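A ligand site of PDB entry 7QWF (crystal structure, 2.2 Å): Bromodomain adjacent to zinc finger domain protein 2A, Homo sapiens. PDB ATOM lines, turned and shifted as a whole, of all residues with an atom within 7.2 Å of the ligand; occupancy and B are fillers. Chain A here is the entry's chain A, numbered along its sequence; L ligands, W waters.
Residues that only touch the ligand: Trp 23 (3.3 Å), Phe 25 (3.8 Å), Val 29 (3.5 Å), Val 34 (3.8 Å), Tyr 37 (3.6 Å), Phe 79 (3.4 Å) and Val 86 (3.7 Å).
Hydrophobic or aromatic side chains that line the ligand: Pro 24, Phe 25, Val 29, Val 34, Tyr 37, Phe 79 and Val 86.
Within 4 Å of the ligand: Trp 23, Pro 24, Phe 25, Glu 27, Val 29, Val 34, Tyr 37, Phe 79, Asn 80 and Val 86.
The side-chain amide nitrogen of Asn 80 lies within hydrogen-bond range of the backbone carbonyl oxygen of Cys 76 (3.0 Å).
The backbone carbonyl oxygen (O) of Val 86 lies within hydrogen-bond range of the side-chain sulfur (SG) of Cys 76.
Water W5 lies within hydrogen-bond range of an oxygen (O1) of the ligand (2.6 Å), the side-chain hydroxyl (OH) of Tyr 37 (3.0 Å) and the backbone carbonyl oxygen (O) of Asn 75 (3.5 Å).
Water W2 lies within hydrogen-bond range of O of Glu 27 (3.1 Å), N3 of the ligand (3.1 Å) and O of Pro 24 (3.2 Å).
An oxygen (O1) of the ligand lies within hydrogen-bond range of the side-chain amide nitrogen (ND2) of Asn 80.
A nitrogen (N1) of the ligand is in hydrogen-bond range of the backbone carbonyl oxygen (O) of Pro 24, at 3.0 Å.
OE2 of Glu 27 lies within salt-bridge range of N2 of the ligand, 3.5 Å away.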
ATOM      1  N   ALA A  22      13.559  -7.457 -30.700  1.00  0.00           N
ATOM      2  CA  ALA A  22      14.395  -6.551 -29.924  1.00  0.00           C
ATOM      3  C   ALA A  22      13.712  -5.248 -29.589  1.00  0.00           C
ATOM      4  O   ALA A  22      14.195  -4.529 -28.704  1.00  0.00           O
ATOM      5  CB  ALA A  22      15.685  -6.225 -30.689  1.00  0.00           C
ATOM      6  N   TRP A  23      12.598  -4.939 -30.230  1.00  0.00           N
ATOM      7  CA  TRP A  23      11.965  -3.638 -30.116  1.00  0.00           C
ATOM      8  C   TRP A  23      11.789  -3.149 -28.664  1.00  0.00           C
ATOM      9  O   TRP A  23      11.901  -1.946 -28.457  1.00  0.00           O
ATOM     10  CB  TRP A  23      10.621  -3.630 -30.845  1.00  0.00           C
ATOM     11  CG  TRP A  23       9.676  -4.661 -30.390  1.00  0.00           C
ATOM     12  CD1 TRP A  23       9.525  -5.907 -30.906  1.00  0.00           C
ATOM     13  CD2 TRP A  23       8.714  -4.547 -29.338  1.00  0.00           C
ATOM     14  NE1 TRP A  23       8.543  -6.583 -30.241  1.00  0.00           N
ATOM     15  CE2 TRP A  23       8.032  -5.773 -29.264  1.00  0.00           C
ATOM     16  CE3 TRP A  23       8.383  -3.527 -28.438  1.00  0.00           C
ATOM     17  CZ2 TRP A  23       7.020  -6.015 -28.324  1.00  0.00           C
ATOM     18  CZ3 TRP A  23       7.379  -3.768 -27.514  1.00  0.00           C
ATOM     19  CH2 TRP A  23       6.714  -4.998 -27.463  1.00  0.00           C
ATOM     20  N   PRO A  24      11.551  -4.000 -27.648  1.00  0.00           N
ATOM     21  CA  PRO A  24      11.442  -3.441 -26.291  1.00  0.00           C
ATOM     22  C   PRO A  24      12.758  -3.015 -25.696  1.00  0.00           C
ATOM     23  O   PRO A  24      12.744  -2.240 -24.719  1.00  0.00           O
ATOM     24  CB  PRO A  24      10.845  -4.603 -25.479  1.00  0.00           C
ATOM     25  CG  PRO A  24      10.381  -5.610 -26.487  1.00  0.00           C
ATOM     26  CD  PRO A  24      11.294  -5.444 -27.633  1.00  0.00           C
ATOM     27  N   PHE A  25      13.894  -3.441 -26.243  1.00  0.00           N
ATOM     28  CA  PHE A  25      15.169  -3.316 -25.563  1.00  0.00           C
ATOM     29  C   PHE A  25      16.168  -2.414 -26.281  1.00  0.00           C
ATOM     30  O   PHE A  25      17.344  -2.385 -25.900  1.00  0.00           O
ATOM     31  CB  PHE A  25      15.771  -4.707 -25.350  1.00  0.00           C
ATOM     32  CG  PHE A  25      14.774  -5.690 -24.846  1.00  0.00           C
ATOM     33  CD1 PHE A  25      14.281  -5.599 -23.554  1.00  0.00           C
ATOM     34  CD2 PHE A  25      14.283  -6.690 -25.678  1.00  0.00           C
ATOM     35  CE1 PHE A  25      13.349  -6.493 -23.066  1.00  0.00           C
ATOM     36  CE2 PHE A  25      13.350  -7.591 -25.212  1.00  0.00           C
ATOM     37  CZ  PHE A  25      12.878  -7.497 -23.909  1.00  0.00           C
ATOM     38  N   LEU A  26      15.727  -1.649 -27.279  1.00  0.00           N
ATOM     39  CA  LEU A  26      16.640  -0.825 -28.049  1.00  0.00           C
ATOM     40  C   LEU A  26      17.059   0.438 -27.279  1.00  0.00           C
ATOM     41  O   LEU A  26      18.167   0.946 -27.469  1.00  0.00           O
ATOM     42  CB  LEU A  26      16.008  -0.463 -29.396  1.00  0.00           C
ATOM     43  CG  LEU A  26      15.650  -1.656 -30.304  1.00  0.00           C
ATOM     44  CD1 LEU A  26      14.928  -1.252 -31.595  1.00  0.00           C
ATOM     45  CD2 LEU A  26      16.912  -2.416 -30.632  1.00  0.00           C
ATOM     46  N   GLU A  27      16.202   0.945 -26.415  1.00  0.00           N
ATOM     47  CA  GLU A  27      16.467   2.183 -25.679  1.00  0.00           C
ATOM     48  C   GLU A  27      16.081   2.002 -24.230  1.00  0.00           C
ATOM     49  O   GLU A  27      15.316   1.087 -23.888  1.00  0.00           O
ATOM     50  CB  GLU A  27      15.687   3.353 -26.308  1.00  0.00           C
ATOM     51  CG  GLU A  27      14.164   3.281 -26.161  1.00  0.00           C
ATOM     52  CD  GLU A  27      13.454   4.358 -26.978  1.00  0.00           C
ATOM     53  OE1 GLU A  27      14.020   4.832 -27.982  1.00  0.00           O
ATOM     54  OE2 GLU A  27      12.315   4.722 -26.594  1.00  0.00           O
ATOM     55  N   PRO A  28      16.599   2.841 -23.322  1.00  0.00           N
ATOM     56  CA  PRO A  28      16.241   2.715 -21.899  1.00  0.00           C
ATOM     57  C   PRO A  28      14.727   2.765 -21.703  1.00  0.00           C
ATOM     58  O   PRO A  28      14.020   3.447 -22.440  1.00  0.00           O
ATOM     59  CB  PRO A  28      16.918   3.927 -21.244  1.00  0.00           C
ATOM     60  CG  PRO A  28      18.013   4.303 -22.174  1.00  0.00           C
ATOM     61  CD  PRO A  28      17.519   3.971 -23.552  1.00  0.00           C
ATOM     62  N   VAL A  29      14.241   2.033 -20.709  1.00  0.00           N
ATOM     63  CA  VAL A  29      12.858   2.221 -20.297  1.00  0.00           C
ATOM     64  C   VAL A  29      12.706   3.633 -19.709  1.00  0.00           C
ATOM     65  O   VAL A  29      13.544   4.087 -18.924  1.00  0.00           O
ATOM     66  CB  VAL A  29      12.452   1.150 -19.276  1.00  0.00           C
ATOM     67  CG1 VAL A  29      11.062   1.422 -18.749  1.00  0.00           C
ATOM     68  CG2 VAL A  29      12.476  -0.223 -19.931  1.00  0.00           C
ATOM     69  N   ASN A  30      11.654   4.333 -20.118  1.00  0.00           N
ATOM     70  CA  ASN A  30      11.360   5.673 -19.603  1.00  0.00           C
ATOM     71  C   ASN A  30      10.519   5.546 -18.339  1.00  0.00           C
ATOM     72  O   ASN A  30       9.314   5.249 -18.443  1.00  0.00           O
ATOM     73  CB  ASN A  30      10.637   6.516 -20.624  1.00  0.00           C
ATOM     74  CG  ASN A  30      10.469   7.963 -20.171  1.00  0.00           C
ATOM     75  OD1 ASN A  30      10.597   8.284 -18.997  1.00  0.00           O
ATOM     76  ND2 ASN A  30      10.160   8.841 -21.123  1.00  0.00           N
ATOM     77  N   LEU A  33       7.046   7.041 -18.189  1.00  0.00           N
ATOM     78  CA  LEU A  33       5.983   6.378 -18.927  1.00  0.00           C
ATOM     79  C   LEU A  33       5.494   5.100 -18.280  1.00  0.00           C
ATOM     80  O   LEU A  33       4.375   4.664 -18.581  1.00  0.00           O
ATOM     81  CB  LEU A  33       6.454   6.056 -20.343  1.00  0.00           C
ATOM     82  CG  LEU A  33       6.762   7.330 -21.114  1.00  0.00           C
ATOM     83  CD1 LEU A  33       7.480   6.994 -22.402  1.00  0.00           C
ATOM     84  CD2 LEU A  33       5.474   8.111 -21.368  1.00  0.00           C
ATOM     85  N   VAL A  34       6.281   4.471 -17.426  1.00  0.00           N
ATOM     86  CA  VAL A  34       5.924   3.166 -16.890  1.00  0.00           C
ATOM     87  C   VAL A  34       5.805   3.284 -15.381  1.00  0.00           C
ATOM     88  O   VAL A  34       6.820   3.389 -14.684  1.00  0.00           O
ATOM     89  CB  VAL A  34       6.932   2.080 -17.280  1.00  0.00           C
ATOM     90  CG1 VAL A  34       6.377   0.718 -16.902  1.00  0.00           C
ATOM     91  CG2 VAL A  34       7.240   2.142 -18.768  1.00  0.00           C
ATOM     92  N   SER A  35       4.576   3.231 -14.882  1.00  0.00           N
ATOM     93  CA  SER A  35       4.333   3.295 -13.448  1.00  0.00           C
ATOM     94  C   SER A  35       5.058   2.179 -12.718  1.00  0.00           C
ATOM     95  O   SER A  35       5.030   1.022 -13.138  1.00  0.00           O
ATOM     96  CB  SER A  35       2.831   3.224 -13.160  1.00  0.00           C
ATOM     97  OG  SER A  35       2.591   3.110 -11.761  1.00  0.00           O
ATOM     98  N   TYR A  37       8.181   1.428 -12.399  1.00  0.00           N
ATOM     99  CA  TYR A  37       9.391   0.813 -12.928  1.00  0.00           C
ATOM    100  C   TYR A  37      10.619   1.178 -12.091  1.00  0.00           C
ATOM    101  O   TYR A  37      11.432   0.312 -11.747  1.00  0.00           O
ATOM    102  CB  TYR A  37       9.616   1.227 -14.383  1.00  0.00           C
ATOM    103  CG  TYR A  37      10.685   0.392 -15.062  1.00  0.00           C
ATOM    104  CD1 TYR A  37      10.375  -0.828 -15.662  1.00  0.00           C
ATOM    105  CD2 TYR A  37      12.005   0.838 -15.132  1.00  0.00           C
ATOM    106  CE1 TYR A  37      11.340  -1.601 -16.291  1.00  0.00           C
ATOM    107  CE2 TYR A  37      12.975   0.087 -15.768  1.00  0.00           C
ATOM    108  CZ  TYR A  37      12.638  -1.130 -16.343  1.00  0.00           C
ATOM    109  OH  TYR A  37      13.620  -1.866 -16.953  1.00  0.00           O
ATOM    110  N   ILE A  41      12.902  -1.890 -10.541  1.00  0.00           N
ATOM    111  CA  ILE A  41      14.114  -2.258 -11.271  1.00  0.00           C
ATOM    112  C   ILE A  41      15.241  -1.343 -10.808  1.00  0.00           C
ATOM    113  O   ILE A  41      15.276  -0.178 -11.182  1.00  0.00           O
ATOM    114  CB  ILE A  41      13.903  -2.177 -12.784  1.00  0.00           C
ATOM    115  CG1 ILE A  41      12.835  -3.183 -13.227  1.00  0.00           C
ATOM    116  CG2 ILE A  41      15.230  -2.369 -13.517  1.00  0.00           C
ATOM    117  CD1 ILE A  41      13.269  -4.636 -13.040  1.00  0.00           C
ATOM    118  N   MET A  45      18.851  -1.674 -17.783  1.00  0.00           N
ATOM    119  CA  MET A  45      19.833  -1.958 -18.809  1.00  0.00           C
ATOM    120  C   MET A  45      19.097  -2.186 -20.124  1.00  0.00           C
ATOM    121  O   MET A  45      17.947  -2.626 -20.142  1.00  0.00           O
ATOM    122  CB  MET A  45      20.707  -3.166 -18.422  1.00  0.00           C
ATOM    123  CG  MET A  45      21.833  -3.485 -19.411  1.00  0.00           C
ATOM    124  SD  MET A  45      22.939  -2.107 -19.783  1.00  0.00           S
ATOM    125  CE  MET A  45      23.339  -1.530 -18.142  1.00  0.00           C
ATOM    126  N   ASP A  46      19.751  -1.826 -21.212  1.00  0.00           N
ATOM    127  CA  ASP A  46      19.154  -1.904 -22.533  1.00  0.00           C
ATOM    128  C   ASP A  46      20.263  -2.031 -23.571  1.00  0.00           C
ATOM    129  O   ASP A  46      21.445  -1.864 -23.270  1.00  0.00           O
ATOM    130  CB  ASP A  46      18.264  -0.700 -22.818  1.00  0.00           C
ATOM    131  CG  ASP A  46      19.045   0.578 -22.928  1.00  0.00           C
ATOM    132  OD1 ASP A  46      19.322   1.204 -21.871  1.00  0.00           O
ATOM    133  OD2 ASP A  46      19.405   0.957 -24.053  1.00  0.00           O
ATOM    134  N   VAL A  72      19.506  -7.280 -18.782  1.00  0.00           N
ATOM    135  CA  VAL A  72      18.380  -6.856 -19.594  1.00  0.00           C
ATOM    136  C   VAL A  72      17.221  -7.823 -19.416  1.00  0.00           C
ATOM    137  O   VAL A  72      16.087  -7.422 -19.098  1.00  0.00           O
ATOM    138  CB  VAL A  72      18.770  -6.731 -21.072  1.00  0.00           C
ATOM    139  CG1 VAL A  72      17.538  -6.452 -21.925  1.00  0.00           C
ATOM    140  CG2 VAL A  72      19.786  -5.644 -21.258  1.00  0.00           C
ATOM    141  N   ASN A  75      15.704  -8.067 -15.733  1.00  0.00           N
ATOM    142  CA  ASN A  75      14.777  -6.957 -15.533  1.00  0.00           C
ATOM    143  C   ASN A  75      13.465  -7.202 -16.251  1.00  0.00           C
ATOM    144  O   ASN A  75      12.378  -7.005 -15.688  1.00  0.00           O
ATOM    145  CB  ASN A  75      15.388  -5.649 -16.012  1.00  0.00           C
ATOM    146  CG  ASN A  75      16.556  -5.208 -15.153  1.00  0.00           C
ATOM    147  OD1 ASN A  75      16.743  -5.686 -14.034  1.00  0.00           O
ATOM    148  ND2 ASN A  75      17.346  -4.300 -15.684  1.00  0.00           N
ATOM    149  N   CYS A  76      13.556  -7.636 -17.519  1.00  0.00           N
ATOM    150  CA  CYS A  76      12.354  -7.913 -18.288  1.00  0.00           C
ATOM    151  C   CYS A  76      11.418  -8.862 -17.536  1.00  0.00           C
ATOM    152  O   CYS A  76      10.214  -8.625 -17.464  1.00  0.00           O
ATOM    153  CB  CYS A  76      12.737  -8.515 -19.641  1.00  0.00           C
ATOM    154  SG  CYS A  76      11.317  -8.641 -20.687  1.00  0.00           S
ATOM    155  N   GLN A  77      11.979  -9.930 -16.969  1.00  0.00           N
ATOM    156  CA  GLN A  77      11.152 -10.939 -16.310  1.00  0.00           C
ATOM    157  C   GLN A  77      10.686 -10.501 -14.937  1.00  0.00           C
ATOM    158  O   GLN A  77       9.655 -10.974 -14.459  1.00  0.00           O
ATOM    159  CB  GLN A  77      11.911 -12.260 -16.206  1.00  0.00           C
ATOM    160  CG  GLN A  77      12.108 -12.970 -17.553  1.00  0.00           C
ATOM    161  CD  GLN A  77      13.049 -14.141 -17.440  1.00  0.00           C
ATOM    162  OE1 GLN A  77      12.624 -15.252 -17.153  1.00  0.00           O
ATOM    163  NE2 GLN A  77      14.342 -13.897 -17.634  1.00  0.00           N
ATOM    164  N   PHE A  79       9.789  -7.349 -14.165  1.00  0.00           N
ATOM    165  CA  PHE A  79       8.724  -6.370 -14.287  1.00  0.00           C
ATOM    166  C   PHE A  79       7.540  -6.828 -15.130  1.00  0.00           C
ATOM    167  O   PHE A  79       6.401  -6.463 -14.818  1.00  0.00           O
ATOM    168  CB  PHE A  79       9.257  -5.072 -14.884  1.00  0.00           C
ATOM    169  CG  PHE A  79       8.341  -3.910 -14.693  1.00  0.00           C
ATOM    170  CD1 PHE A  79       8.387  -3.151 -13.531  1.00  0.00           C
ATOM    171  CD2 PHE A  79       7.394  -3.591 -15.651  1.00  0.00           C
ATOM    172  CE1 PHE A  79       7.527  -2.088 -13.341  1.00  0.00           C
ATOM    173  CE2 PHE A  79       6.532  -2.514 -15.461  1.00  0.00           C
ATOM    174  CZ  PHE A  79       6.609  -1.764 -14.303  1.00  0.00           C
ATOM    175  N   ASN A  80       7.766  -7.603 -16.202  1.00  0.00           N
ATOM    176  CA  ASN A  80       6.725  -7.915 -17.173  1.00  0.00           C
ATOM    177  C   ASN A  80       6.221  -9.337 -17.002  1.00  0.00           C
ATOM    178  O   ASN A  80       6.992 -10.258 -16.730  1.00  0.00           O
ATOM    179  CB  ASN A  80       7.246  -7.720 -18.591  1.00  0.00           C
ATOM    180  CG  ASN A  80       7.758  -6.339 -18.821  1.00  0.00           C
ATOM    181  OD1 ASN A  80       6.991  -5.403 -19.050  1.00  0.00           O
ATOM    182  ND2 ASN A  80       9.079  -6.188 -18.783  1.00  0.00           N
ATOM    183  N   SER A  84       2.850 -11.129 -21.303  1.00  0.00           N
ATOM    184  CA  SER A  84       2.777  -9.791 -21.877  1.00  0.00           C
ATOM    185  C   SER A  84       3.586  -9.733 -23.158  1.00  0.00           C
ATOM    186  O   SER A  84       4.480 -10.546 -23.397  1.00  0.00           O
ATOM    187  CB  SER A  84       3.303  -8.745 -20.893  1.00  0.00           C
ATOM    188  OG  SER A  84       4.661  -9.002 -20.565  1.00  0.00           O
ATOM    189  N   VAL A  86       5.822  -7.536 -24.067  1.00  0.00           N
ATOM    190  CA  VAL A  86       7.224  -7.299 -23.733  1.00  0.00           C
ATOM    191  C   VAL A  86       7.839  -8.545 -23.131  1.00  0.00           C
ATOM    192  O   VAL A  86       8.997  -8.872 -23.410  1.00  0.00           O
ATOM    193  CB  VAL A  86       7.341  -6.095 -22.784  1.00  0.00           C
ATOM    194  CG1 VAL A  86       8.734  -5.999 -22.241  1.00  0.00           C
ATOM    195  CG2 VAL A  86       6.968  -4.816 -23.514  1.00  0.00           C
HETATM  196  C1  LIG L   1       6.092  -2.060 -21.271  1.00  0.00           C
HETATM  197  C2  LIG L   1       7.200  -1.016 -21.428  1.00  0.00           C
HETATM  198  C3  LIG L   1       8.569  -1.594 -21.808  1.00  0.00           C
HETATM  199  C4  LIG L   1       9.123  -1.462 -23.066  1.00  0.00           C
HETATM  200  C5  LIG L   1      10.563  -2.574 -21.840  1.00  0.00           C
HETATM  201  C6  LIG L   1      11.864  -3.312 -21.516  1.00  0.00           C
HETATM  202  C7  LIG L   1       9.480  -2.288 -21.014  1.00  0.00           C
HETATM  203  C8  LIG L   1       9.383  -2.703 -19.527  1.00  0.00           C
HETATM  204  C9  LIG L   1       8.371  -2.094 -18.555  1.00  0.00           C
HETATM  205  C10 LIG L   1       8.567  -0.796 -24.332  1.00  0.00           C
HETATM  206  C11 LIG L   1       7.214  -0.794 -24.774  1.00  0.00           C
HETATM  207  C12 LIG L   1       8.660   0.410 -26.387  1.00  0.00           C
HETATM  208  C13 LIG L   1       9.210   1.213 -27.562  1.00  0.00           C
HETATM  209  C14 LIG L   1      10.720   1.457 -27.459  1.00  0.00           C
HETATM  210  C15 LIG L   1      11.917   1.140 -29.515  1.00  0.00           C
HETATM  211  N1  LIG L   1      10.316  -2.054 -23.042  1.00  0.00           N
HETATM  212  N2  LIG L   1      11.242   2.099 -28.658  1.00  0.00           N
HETATM  213  N3  LIG L   1       9.416  -0.085 -25.315  1.00  0.00           N
HETATM  214  O1  LIG L   1      10.140  -3.494 -19.061  1.00  0.00           O
HETATM  215  S1  LIG L   1       7.101   0.001 -26.161  1.00  0.00           S
HETATM  216  O   HOH W   1      14.096  -1.224 -22.796  1.00  0.00           O
HETATM  217  O   HOH W   2      12.241   0.947 -24.439  1.00  0.00           O
HETATM  218  O   HOH W   3      15.246  -2.948 -20.789  1.00  0.00           O
HETATM  219  O   HOH W   4      13.538  -0.060 -26.992  1.00  0.00           O
HETATM  220  O   HOH W   5      12.305  -4.333 -17.896  1.00  0.00           O
